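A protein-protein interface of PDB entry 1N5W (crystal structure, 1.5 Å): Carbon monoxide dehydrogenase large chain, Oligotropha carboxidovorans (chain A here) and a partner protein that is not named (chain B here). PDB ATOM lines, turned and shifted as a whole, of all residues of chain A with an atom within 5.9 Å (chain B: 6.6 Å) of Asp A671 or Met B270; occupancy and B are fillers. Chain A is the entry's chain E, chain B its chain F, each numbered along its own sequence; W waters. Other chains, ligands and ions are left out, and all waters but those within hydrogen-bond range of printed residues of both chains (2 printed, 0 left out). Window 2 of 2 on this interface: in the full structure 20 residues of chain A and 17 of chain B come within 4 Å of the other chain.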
ATOM      1  N   ARG A 476      23.758  19.623  21.600  1.00  0.00           N
ATOM      2  CA  ARG A 476      22.872  18.543  21.164  1.00  0.00           C
ATOM      3  C   ARG A 476      22.298  18.779  19.781  1.00  0.00           C
ATOM      4  O   ARG A 476      21.443  18.013  19.308  1.00  0.00           O
ATOM      5  CB  ARG A 476      21.769  18.334  22.194  1.00  0.00           C
ATOM      6  CG  ARG A 476      22.328  18.048  23.617  1.00  0.00           C
ATOM      7  CD  ARG A 476      23.209  16.819  23.641  1.00  0.00           C
ATOM      8  NE  ARG A 476      22.478  15.619  23.291  1.00  0.00           N
ATOM      9  CZ  ARG A 476      23.028  14.438  23.038  1.00  0.00           C
ATOM     10  NH1 ARG A 476      24.336  14.311  22.898  1.00  0.00           N
ATOM     11  NH2 ARG A 476      22.275  13.399  22.789  1.00  0.00           N
ATOM     12  N   ASP A 669      17.855  18.848  16.406  1.00  0.00           N
ATOM     13  CA  ASP A 669      17.966  18.484  17.848  1.00  0.00           C
ATOM     14  C   ASP A 669      17.981  16.973  17.911  1.00  0.00           C
ATOM     15  O   ASP A 669      16.956  16.345  17.596  1.00  0.00           O
ATOM     16  CB  ASP A 669      16.774  19.093  18.625  1.00  0.00           C
ATOM     17  CG  ASP A 669      16.772  18.816  20.107  1.00  0.00           C
ATOM     18  OD1 ASP A 669      17.272  17.741  20.550  1.00  0.00           O
ATOM     19  OD2 ASP A 669      16.351  19.697  20.902  1.00  0.00           O
ATOM     20  N   VAL A 670      19.114  16.329  18.245  1.00  0.00           N
ATOM     21  CA  VAL A 670      19.146  14.881  18.161  1.00  0.00           C
ATOM     22  C   VAL A 670      18.314  14.192  19.248  1.00  0.00           C
ATOM     23  O   VAL A 670      18.005  13.008  19.107  1.00  0.00           O
ATOM     24  CB  VAL A 670      20.581  14.346  18.181  1.00  0.00           C
ATOM     25  CG1 VAL A 670      21.448  14.890  17.105  1.00  0.00           C
ATOM     26  CG2 VAL A 670      21.227  14.498  19.581  1.00  0.00           C
ATOM     27  N   ASP A 671      17.951  14.917  20.330  1.00  0.00           N
ATOM     28  CA  ASP A 671      17.243  14.321  21.446  1.00  0.00           C
ATOM     29  C   ASP A 671      15.740  14.259  21.189  1.00  0.00           C
ATOM     30  O   ASP A 671      15.094  13.326  21.733  1.00  0.00           O
ATOM     31  CB  ASP A 671      17.582  15.093  22.696  1.00  0.00           C
ATOM     32  CG  ASP A 671      19.016  14.873  23.143  1.00  0.00           C
ATOM     33  OD1 ASP A 671      19.563  13.730  23.034  1.00  0.00           O
ATOM     34  OD2 ASP A 671      19.669  15.836  23.596  1.00  0.00           O
ATOM     35  N   THR A 672      15.181  15.178  20.378  1.00  0.00           N
ATOM     36  CA  THR A 672      13.764  15.147  20.041  1.00  0.00           C
ATOM     37  C   THR A 672      13.512  14.767  18.606  1.00  0.00           C
ATOM     38  O   THR A 672      12.412  14.330  18.275  1.00  0.00           O
ATOM     39  CB  THR A 672      13.072  16.499  20.281  1.00  0.00           C
ATOM     40  OG1 THR A 672      13.750  17.473  19.479  1.00  0.00           O
ATOM     41  CG2 THR A 672      13.082  16.942  21.754  1.00  0.00           C
ATOM     42  N   GLY A 673      14.530  14.856  17.761  1.00  0.00           N
ATOM     43  CA  GLY A 673      14.378  14.657  16.325  1.00  0.00           C
ATOM     44  C   GLY A 673      13.900  15.866  15.564  1.00  0.00           C
ATOM     45  O   GLY A 673      13.659  15.759  14.339  1.00  0.00           O
ATOM     46  N   TRP A 799      14.309  10.902  15.653  1.00  0.00           N
ATOM     47  CA  TRP A 799      14.644  10.399  16.989  1.00  0.00           C
ATOM     48  C   TRP A 799      15.124   8.962  16.845  1.00  0.00           C
ATOM     49  O   TRP A 799      16.079   8.564  17.533  1.00  0.00           O
ATOM     50  CB  TRP A 799      13.443  10.469  17.911  1.00  0.00           C
ATOM     51  CG  TRP A 799      13.741   9.904  19.284  1.00  0.00           C
ATOM     52  CD1 TRP A 799      14.216  10.605  20.371  1.00  0.00           C
ATOM     53  CD2 TRP A 799      13.465   8.591  19.749  1.00  0.00           C
ATOM     54  NE1 TRP A 799      14.357   9.761  21.445  1.00  0.00           N
ATOM     55  CE2 TRP A 799      13.880   8.526  21.095  1.00  0.00           C
ATOM     56  CE3 TRP A 799      12.937   7.443  19.155  1.00  0.00           C
ATOM     57  CZ2 TRP A 799      13.794   7.377  21.847  1.00  0.00           C
ATOM     58  CZ3 TRP A 799      12.910   6.249  19.899  1.00  0.00           C
ATOM     59  CH2 TRP A 799      13.252   6.257  21.256  1.00  0.00           C
ATOM     60  N   LEU A 807      22.880   7.839  20.557  1.00  0.00           N
ATOM     61  CA  LEU A 807      23.022   9.232  20.959  1.00  0.00           C
ATOM     62  C   LEU A 807      22.288   9.570  22.246  1.00  0.00           C
ATOM     63  O   LEU A 807      22.468  10.645  22.799  1.00  0.00           O
ATOM     64  CB  LEU A 807      22.557  10.158  19.834  1.00  0.00           C
ATOM     65  CG  LEU A 807      23.143   9.970  18.453  1.00  0.00           C
ATOM     66  CD1 LEU A 807      22.702  11.050  17.512  1.00  0.00           C
ATOM     67  CD2 LEU A 807      24.647   9.949  18.559  1.00  0.00           C
ATOM     68  N   HIS A 808      21.419   8.692  22.718  1.00  0.00           N
ATOM     69  CA  HIS A 808      20.548   9.044  23.841  1.00  0.00           C
ATOM     70  C   HIS A 808      21.006   8.510  25.207  1.00  0.00           C
ATOM     71  O   HIS A 808      20.207   8.536  26.136  1.00  0.00           O
ATOM     72  CB  HIS A 808      19.095   8.665  23.515  1.00  0.00           C
ATOM     73  CG  HIS A 808      18.557   9.332  22.293  1.00  0.00           C
ATOM     74  ND1 HIS A 808      17.678   8.720  21.414  1.00  0.00           N
ATOM     75  CD2 HIS A 808      18.765  10.580  21.814  1.00  0.00           C
ATOM     76  CE1 HIS A 808      17.366   9.583  20.457  1.00  0.00           C
ATOM     77  NE2 HIS A 808      18.035  10.714  20.669  1.00  0.00           N
ATOM     78  N   LEU B 186       5.214  19.268  22.650  1.00  0.00           N
ATOM     79  CA  LEU B 186       5.845  18.785  21.414  1.00  0.00           C
ATOM     80  C   LEU B 186       4.677  18.387  20.520  1.00  0.00           C
ATOM     81  O   LEU B 186       3.858  17.572  20.898  1.00  0.00           O
ATOM     82  CB  LEU B 186       6.778  17.609  21.691  1.00  0.00           C
ATOM     83  CG  LEU B 186       7.481  16.976  20.501  1.00  0.00           C
ATOM     84  CD1 LEU B 186       8.494  17.952  19.806  1.00  0.00           C
ATOM     85  CD2 LEU B 186       8.208  15.710  20.856  1.00  0.00           C
ATOM     86  N   THR B 195       2.303  15.266  20.795  1.00  0.00           N
ATOM     87  CA  THR B 195       3.102  14.052  20.860  1.00  0.00           C
ATOM     88  C   THR B 195       3.329  13.707  22.333  1.00  0.00           C
ATOM     89  O   THR B 195       3.149  12.537  22.770  1.00  0.00           O
ATOM     90  CB  THR B 195       4.409  14.281  20.090  1.00  0.00           C
ATOM     91  OG1 THR B 195       4.059  14.570  18.719  1.00  0.00           O
ATOM     92  CG2 THR B 195       5.307  13.041  20.109  1.00  0.00           C
ATOM     93  N   ALA B 196       3.727  14.715  23.108  1.00  0.00           N
ATOM     94  CA  ALA B 196       3.754  14.699  24.571  1.00  0.00           C
ATOM     95  C   ALA B 196       3.792  16.138  25.061  1.00  0.00           C
ATOM     96  O   ALA B 196       4.340  17.006  24.357  1.00  0.00           O
ATOM     97  CB  ALA B 196       4.976  13.952  25.055  1.00  0.00           C
ATOM     98  N   ALA B 197       3.256  16.420  26.235  1.00  0.00           N
ATOM     99  CA  ALA B 197       3.416  17.748  26.843  1.00  0.00           C
ATOM    100  C   ALA B 197       3.492  17.608  28.360  1.00  0.00           C
ATOM    101  O   ALA B 197       2.951  16.617  28.945  1.00  0.00           O
ATOM    102  CB  ALA B 197       2.319  18.655  26.414  1.00  0.00           C
ATOM    103  N   ALA B 198       4.166  18.563  28.985  1.00  0.00           N
ATOM    104  CA  ALA B 198       4.247  18.584  30.450  1.00  0.00           C
ATOM    105  C   ALA B 198       3.866  19.958  31.012  1.00  0.00           C
ATOM    106  O   ALA B 198       4.289  20.983  30.503  1.00  0.00           O
ATOM    107  CB  ALA B 198       5.656  18.200  30.899  1.00  0.00           C
ATOM    108  N   VAL B 219      -0.057  11.104  26.870  1.00  0.00           N
ATOM    109  CA  VAL B 219       0.920  10.023  26.940  1.00  0.00           C
ATOM    110  C   VAL B 219       0.359   8.838  27.739  1.00  0.00           C
ATOM    111  O   VAL B 219       1.098   8.009  28.300  1.00  0.00           O
ATOM    112  CB  VAL B 219       2.302  10.520  27.468  1.00  0.00           C
ATOM    113  CG1 VAL B 219       2.972  11.330  26.389  1.00  0.00           C
ATOM    114  CG2 VAL B 219       2.195  11.307  28.745  1.00  0.00           C
ATOM    115  N   GLU B 251       8.193   8.946  33.344  1.00  0.00           N
ATOM    116  CA  GLU B 251       8.198   7.970  32.265  1.00  0.00           C
ATOM    117  C   GLU B 251       7.499   6.695  32.723  1.00  0.00           C
ATOM    118  O   GLU B 251       6.783   6.064  31.923  1.00  0.00           O
ATOM    119  CB  GLU B 251       9.623   7.638  31.826  1.00  0.00           C
ATOM    120  CG  GLU B 251      10.293   8.730  30.966  1.00  0.00           C
ATOM    121  CD  GLU B 251      11.710   8.439  30.582  1.00  0.00           C
ATOM    122  OE1 GLU B 251      12.283   7.433  31.074  1.00  0.00           O
ATOM    123  OE2 GLU B 251      12.261   9.223  29.783  1.00  0.00           O
ATOM    124  N   GLU B 265       7.254   4.173  22.593  1.00  0.00           N
ATOM    125  CA  GLU B 265       8.549   4.348  23.217  1.00  0.00           C
ATOM    126  C   GLU B 265       9.092   5.768  22.999  1.00  0.00           C
ATOM    127  O   GLU B 265       9.671   6.349  23.934  1.00  0.00           O
ATOM    128  CB  GLU B 265       9.558   3.277  22.749  1.00  0.00           C
ATOM    129  CG  GLU B 265       9.828   3.154  21.254  1.00  0.00           C
ATOM    130  CD  GLU B 265       8.838   2.322  20.435  1.00  0.00           C
ATOM    131  OE1 GLU B 265       9.138   2.085  19.218  1.00  0.00           O
ATOM    132  OE2 GLU B 265       7.773   1.912  20.957  1.00  0.00           O
ATOM    133  N   TYR B 266       8.826   6.350  21.821  1.00  0.00           N
ATOM    134  CA  TYR B 266       9.284   7.686  21.542  1.00  0.00           C
ATOM    135  C   TYR B 266       8.485   8.626  22.447  1.00  0.00           C
ATOM    136  O   TYR B 266       9.037   9.552  23.024  1.00  0.00           O
ATOM    137  CB  TYR B 266       9.006   8.054  20.071  1.00  0.00           C
ATOM    138  CG  TYR B 266       9.194   9.519  19.708  1.00  0.00           C
ATOM    139  CD1 TYR B 266      10.413  10.135  19.861  1.00  0.00           C
ATOM    140  CD2 TYR B 266       8.175  10.277  19.130  1.00  0.00           C
ATOM    141  CE1 TYR B 266      10.628  11.426  19.458  1.00  0.00           C
ATOM    142  CE2 TYR B 266       8.401  11.550  18.758  1.00  0.00           C
ATOM    143  CZ  TYR B 266       9.608  12.154  18.928  1.00  0.00           C
ATOM    144  OH  TYR B 266       9.803  13.448  18.542  1.00  0.00           O
ATOM    145  N   ARG B 267       7.181   8.423  22.508  1.00  0.00           N
ATOM    146  CA  ARG B 267       6.338   9.353  23.256  1.00  0.00           C
ATOM    147  C   ARG B 267       6.613   9.314  24.755  1.00  0.00           C
ATOM    148  O   ARG B 267       6.645  10.364  25.371  1.00  0.00           O
ATOM    149  CB  ARG B 267       4.873   9.119  22.906  1.00  0.00           C
ATOM    150  CG  ARG B 267       4.593   9.320  21.434  1.00  0.00           C
ATOM    151  CD  ARG B 267       3.158   9.022  21.053  1.00  0.00           C
ATOM    152  NE  ARG B 267       2.278  10.105  21.488  1.00  0.00           N
ATOM    153  CZ  ARG B 267       0.991  10.172  21.157  1.00  0.00           C
ATOM    154  NH1 ARG B 267       0.403   9.157  20.540  1.00  0.00           N
ATOM    155  NH2 ARG B 267       0.264  11.231  21.427  1.00  0.00           N
ATOM    156  N   THR B 268       6.951   8.146  25.319  1.00  0.00           N
ATOM    157  CA  THR B 268       7.413   8.098  26.696  1.00  0.00           C
ATOM    158  C   THR B 268       8.696   8.917  26.915  1.00  0.00           C
ATOM    159  O   THR B 268       8.789   9.682  27.882  1.00  0.00           O
ATOM    160  CB  THR B 268       7.614   6.629  27.100  1.00  0.00           C
ATOM    161  OG1 THR B 268       6.312   6.000  27.224  1.00  0.00           O
ATOM    162  CG2 THR B 268       8.394   6.496  28.394  1.00  0.00           C
ATOM    163  N   LYS B 269       9.681   8.747  26.030  1.00  0.00           N
ATOM    164  CA  LYS B 269      10.869   9.540  26.142  1.00  0.00           C
ATOM    165  C   LYS B 269      10.552  11.030  26.003  1.00  0.00           C
ATOM    166  O   LYS B 269      11.149  11.900  26.683  1.00  0.00           O
ATOM    167  CB  LYS B 269      11.951   9.100  25.171  1.00  0.00           C
ATOM    168  CG  LYS B 269      12.606   7.762  25.464  1.00  0.00           C
ATOM    169  CD  LYS B 269      13.131   7.508  26.915  1.00  0.00           C
ATOM    170  CE  LYS B 269      14.206   8.452  27.427  1.00  0.00           C
ATOM    171  NZ  LYS B 269      14.617   8.083  28.892  1.00  0.00           N
ATOM    172  N   MET B 270       9.623  11.354  25.114  1.00  0.00           N
ATOM    173  CA  MET B 270       9.317  12.764  24.932  1.00  0.00           C
ATOM    174  C   MET B 270       8.574  13.377  26.125  1.00  0.00           C
ATOM    175  O   MET B 270       8.746  14.565  26.439  1.00  0.00           O
ATOM    176  CB  MET B 270       8.540  13.045  23.623  1.00  0.00           C
ATOM    177  CG  MET B 270       9.335  12.731  22.317  1.00  0.00           C
ATOM    178  SD  MET B 270      10.926  13.659  22.265  1.00  0.00           S
ATOM    179  CE  MET B 270      12.128  12.366  22.819  1.00  0.00           C
ATOM    180  N   ALA B 271       7.794  12.578  26.844  1.00  0.00           N
ATOM    181  CA  ALA B 271       7.226  13.080  28.078  1.00  0.00           C
ATOM    182  C   ALA B 271       8.351  13.524  29.038  1.00  0.00           C
ATOM    183  O   ALA B 271       8.260  14.521  29.743  1.00  0.00           O
ATOM    184  CB  ALA B 271       6.375  12.017  28.732  1.00  0.00           C
ATOM    185  N   GLY B 272       9.426  12.729  29.100  1.00  0.00           N
ATOM    186  CA  GLY B 272      10.561  13.028  29.953  1.00  0.00           C
ATOM    187  C   GLY B 272      11.311  14.252  29.496  1.00  0.00           C
ATOM    188  O   GLY B 272      11.680  15.090  30.298  1.00  0.00           O
ATOM    189  N   VAL B 273      11.449  14.429  28.175  1.00  0.00           N
ATOM    190  CA  VAL B 273      12.205  15.607  27.673  1.00  0.00           C
ATOM    191  C   VAL B 273      11.375  16.898  27.887  1.00  0.00           C
ATOM    192  O   VAL B 273      11.876  17.957  28.290  1.00  0.00           O
ATOM    193  CB  VAL B 273      12.526  15.478  26.193  1.00  0.00           C
ATOM    194  CG1 VAL B 273      13.192  16.764  25.664  1.00  0.00           C
ATOM    195  CG2 VAL B 273      13.490  14.291  25.981  1.00  0.00           C
ATOM    196  N   MET B 274      10.064  16.804  27.643  1.00  0.00           N
ATOM    197  CA  MET B 274       9.217  17.934  27.906  1.00  0.00           C
ATOM    198  C   MET B 274       9.181  18.320  29.388  1.00  0.00           C
ATOM    199  O   MET B 274       9.233  19.508  29.729  1.00  0.00           O
ATOM    200  CB  MET B 274       7.805  17.703  27.362  1.00  0.00           C
ATOM    201  CG  MET B 274       7.629  17.626  25.831  1.00  0.00           C
ATOM    202  SD  MET B 274       8.278  19.030  24.900  1.00  0.00           S
ATOM    203  CE  MET B 274       9.902  18.397  24.401  1.00  0.00           C
ATOM    204  N   LEU B 275       9.169  17.313  30.264  1.00  0.00           N
ATOM    205  CA  LEU B 275       9.215  17.532  31.701  1.00  0.00           C
ATOM    206  C   LEU B 275      10.526  18.266  32.090  1.00  0.00           C
ATOM    207  O   LEU B 275      10.501  19.282  32.782  1.00  0.00           O
ATOM    208  CB  LEU B 275       9.098  16.216  32.469  1.00  0.00           C
ATOM    209  CG  LEU B 275       9.229  16.299  34.006  1.00  0.00           C
ATOM    210  CD1 LEU B 275       8.353  17.393  34.561  1.00  0.00           C
ATOM    211  CD2 LEU B 275       8.888  15.004  34.618  1.00  0.00           C
ATOM    212  N   ARG B 277      12.449  20.174  30.232  1.00  0.00           N
ATOM    213  CA  ARG B 277      12.488  21.534  29.688  1.00  0.00           C
ATOM    214  C   ARG B 277      11.508  22.399  30.476  1.00  0.00           C
ATOM    215  O   ARG B 277      11.778  23.568  30.737  1.00  0.00           O
ATOM    216  CB  ARG B 277      12.205  21.512  28.195  1.00  0.00           C
ATOM    217  CG  ARG B 277      13.302  20.850  27.446  1.00  0.00           C
ATOM    218  CD  ARG B 277      13.041  20.781  25.926  1.00  0.00           C
ATOM    219  NE  ARG B 277      14.156  20.115  25.256  1.00  0.00           N
ATOM    220  CZ  ARG B 277      14.239  19.923  23.935  1.00  0.00           C
ATOM    221  NH1 ARG B 277      13.330  20.464  23.151  1.00  0.00           N
ATOM    222  NH2 ARG B 277      15.281  19.301  23.404  1.00  0.00           N
HETATM  223  O   HOH W   1      18.445  18.426  23.127  1.00  0.00           O
HETATM  224  O   HOH W   2      12.932  20.025  20.187  1.00  0.00           O
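NH2 of Arg B277 is in salt-bridge range of OD2 of Asp A669 (2.7 Å). The backbone carbonyl oxygen (O) of Thr A672 is in hydrogen-bond range of the side-chain hydroxyl (OH) of Tyr B266 (2.8 Å).
NH2 of Arg A476 is in salt-bridge range of OD1 of Asp A671 (2.7 Å). OD1 of Asp A669 is in hydrogen-bond range of N of Asp A671 (2.9 Å). The side-chain carboxylate (OD1) of Asp A669 is in hydrogen-bond range of the backbone NH (N) of Thr A672 (3.3 Å). The indole nitrogen of Trp A799 sits close to a ring nitrogen (ND1) of His A808. OE2 of Glu B251 lies within salt-bridge range of NZ of Lys B269, at 2.8 Å.
CE of Met B270 touches O of Asp A671, 3.3 Å away. CA of Thr A672 touches SD of Met B270 (3.9 Å). Thr A672 touches Val B273. Thr A672 touches Arg B277. Trp A799 touches Tyr B266. CZ2 of Trp A799 touches CG of Lys B269 (3.8 Å). Trp A799 touches Met B270.
Of chain B, only Met B270 comes within 4 Å of Asp A671. Of chain A, only Asp A671 (3.3 Å), Thr A672 (3.9 Å) and Trp A799 (3.7 Å) come within 4 Å of Met B270. Of the printed residues of chain B, Thr A672 touches Tyr B266 (2.8 Å), Met B270 (3.9 Å), Val B273 (3.9 Å) and Arg B277 (3.6 Å). Printed residues of chain A within 4 Å of Arg B277: Asp A669 and Thr A672. The nearest residue of chain B that does not touch Asp A671 is Val B273 (4.6 Å).
Of the 19 printed residues of chain B, 5 touch a printed residue of chain A. Hydrophobic or aromatic side chains of chain B within 4 Å of the printed part of chain A: Tyr B266, Met B270 and Val B273. Hydrophobic or aromatic side chains of chain A within 4 Å of the printed part of chain B: Trp A799. Among the printed residues, Asp or Glu carboxylates within 4 Å of a Lys or Arg side-chain nitrogen of the other chain: Asp A669 with Arg B277.
Water W2 bridges the side-chain hydroxyl of Thr A672 (2.8 Å) and the guanidinium group of Arg B277 (3.0 Å). Water W1 lies within hydrogen-bond range of the side-chain carboxylate (OD2) of Asp A671, the side-chain carboxylate (OD1) of Asp A669 and the guanidinium group (NH2) of Arg B277.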
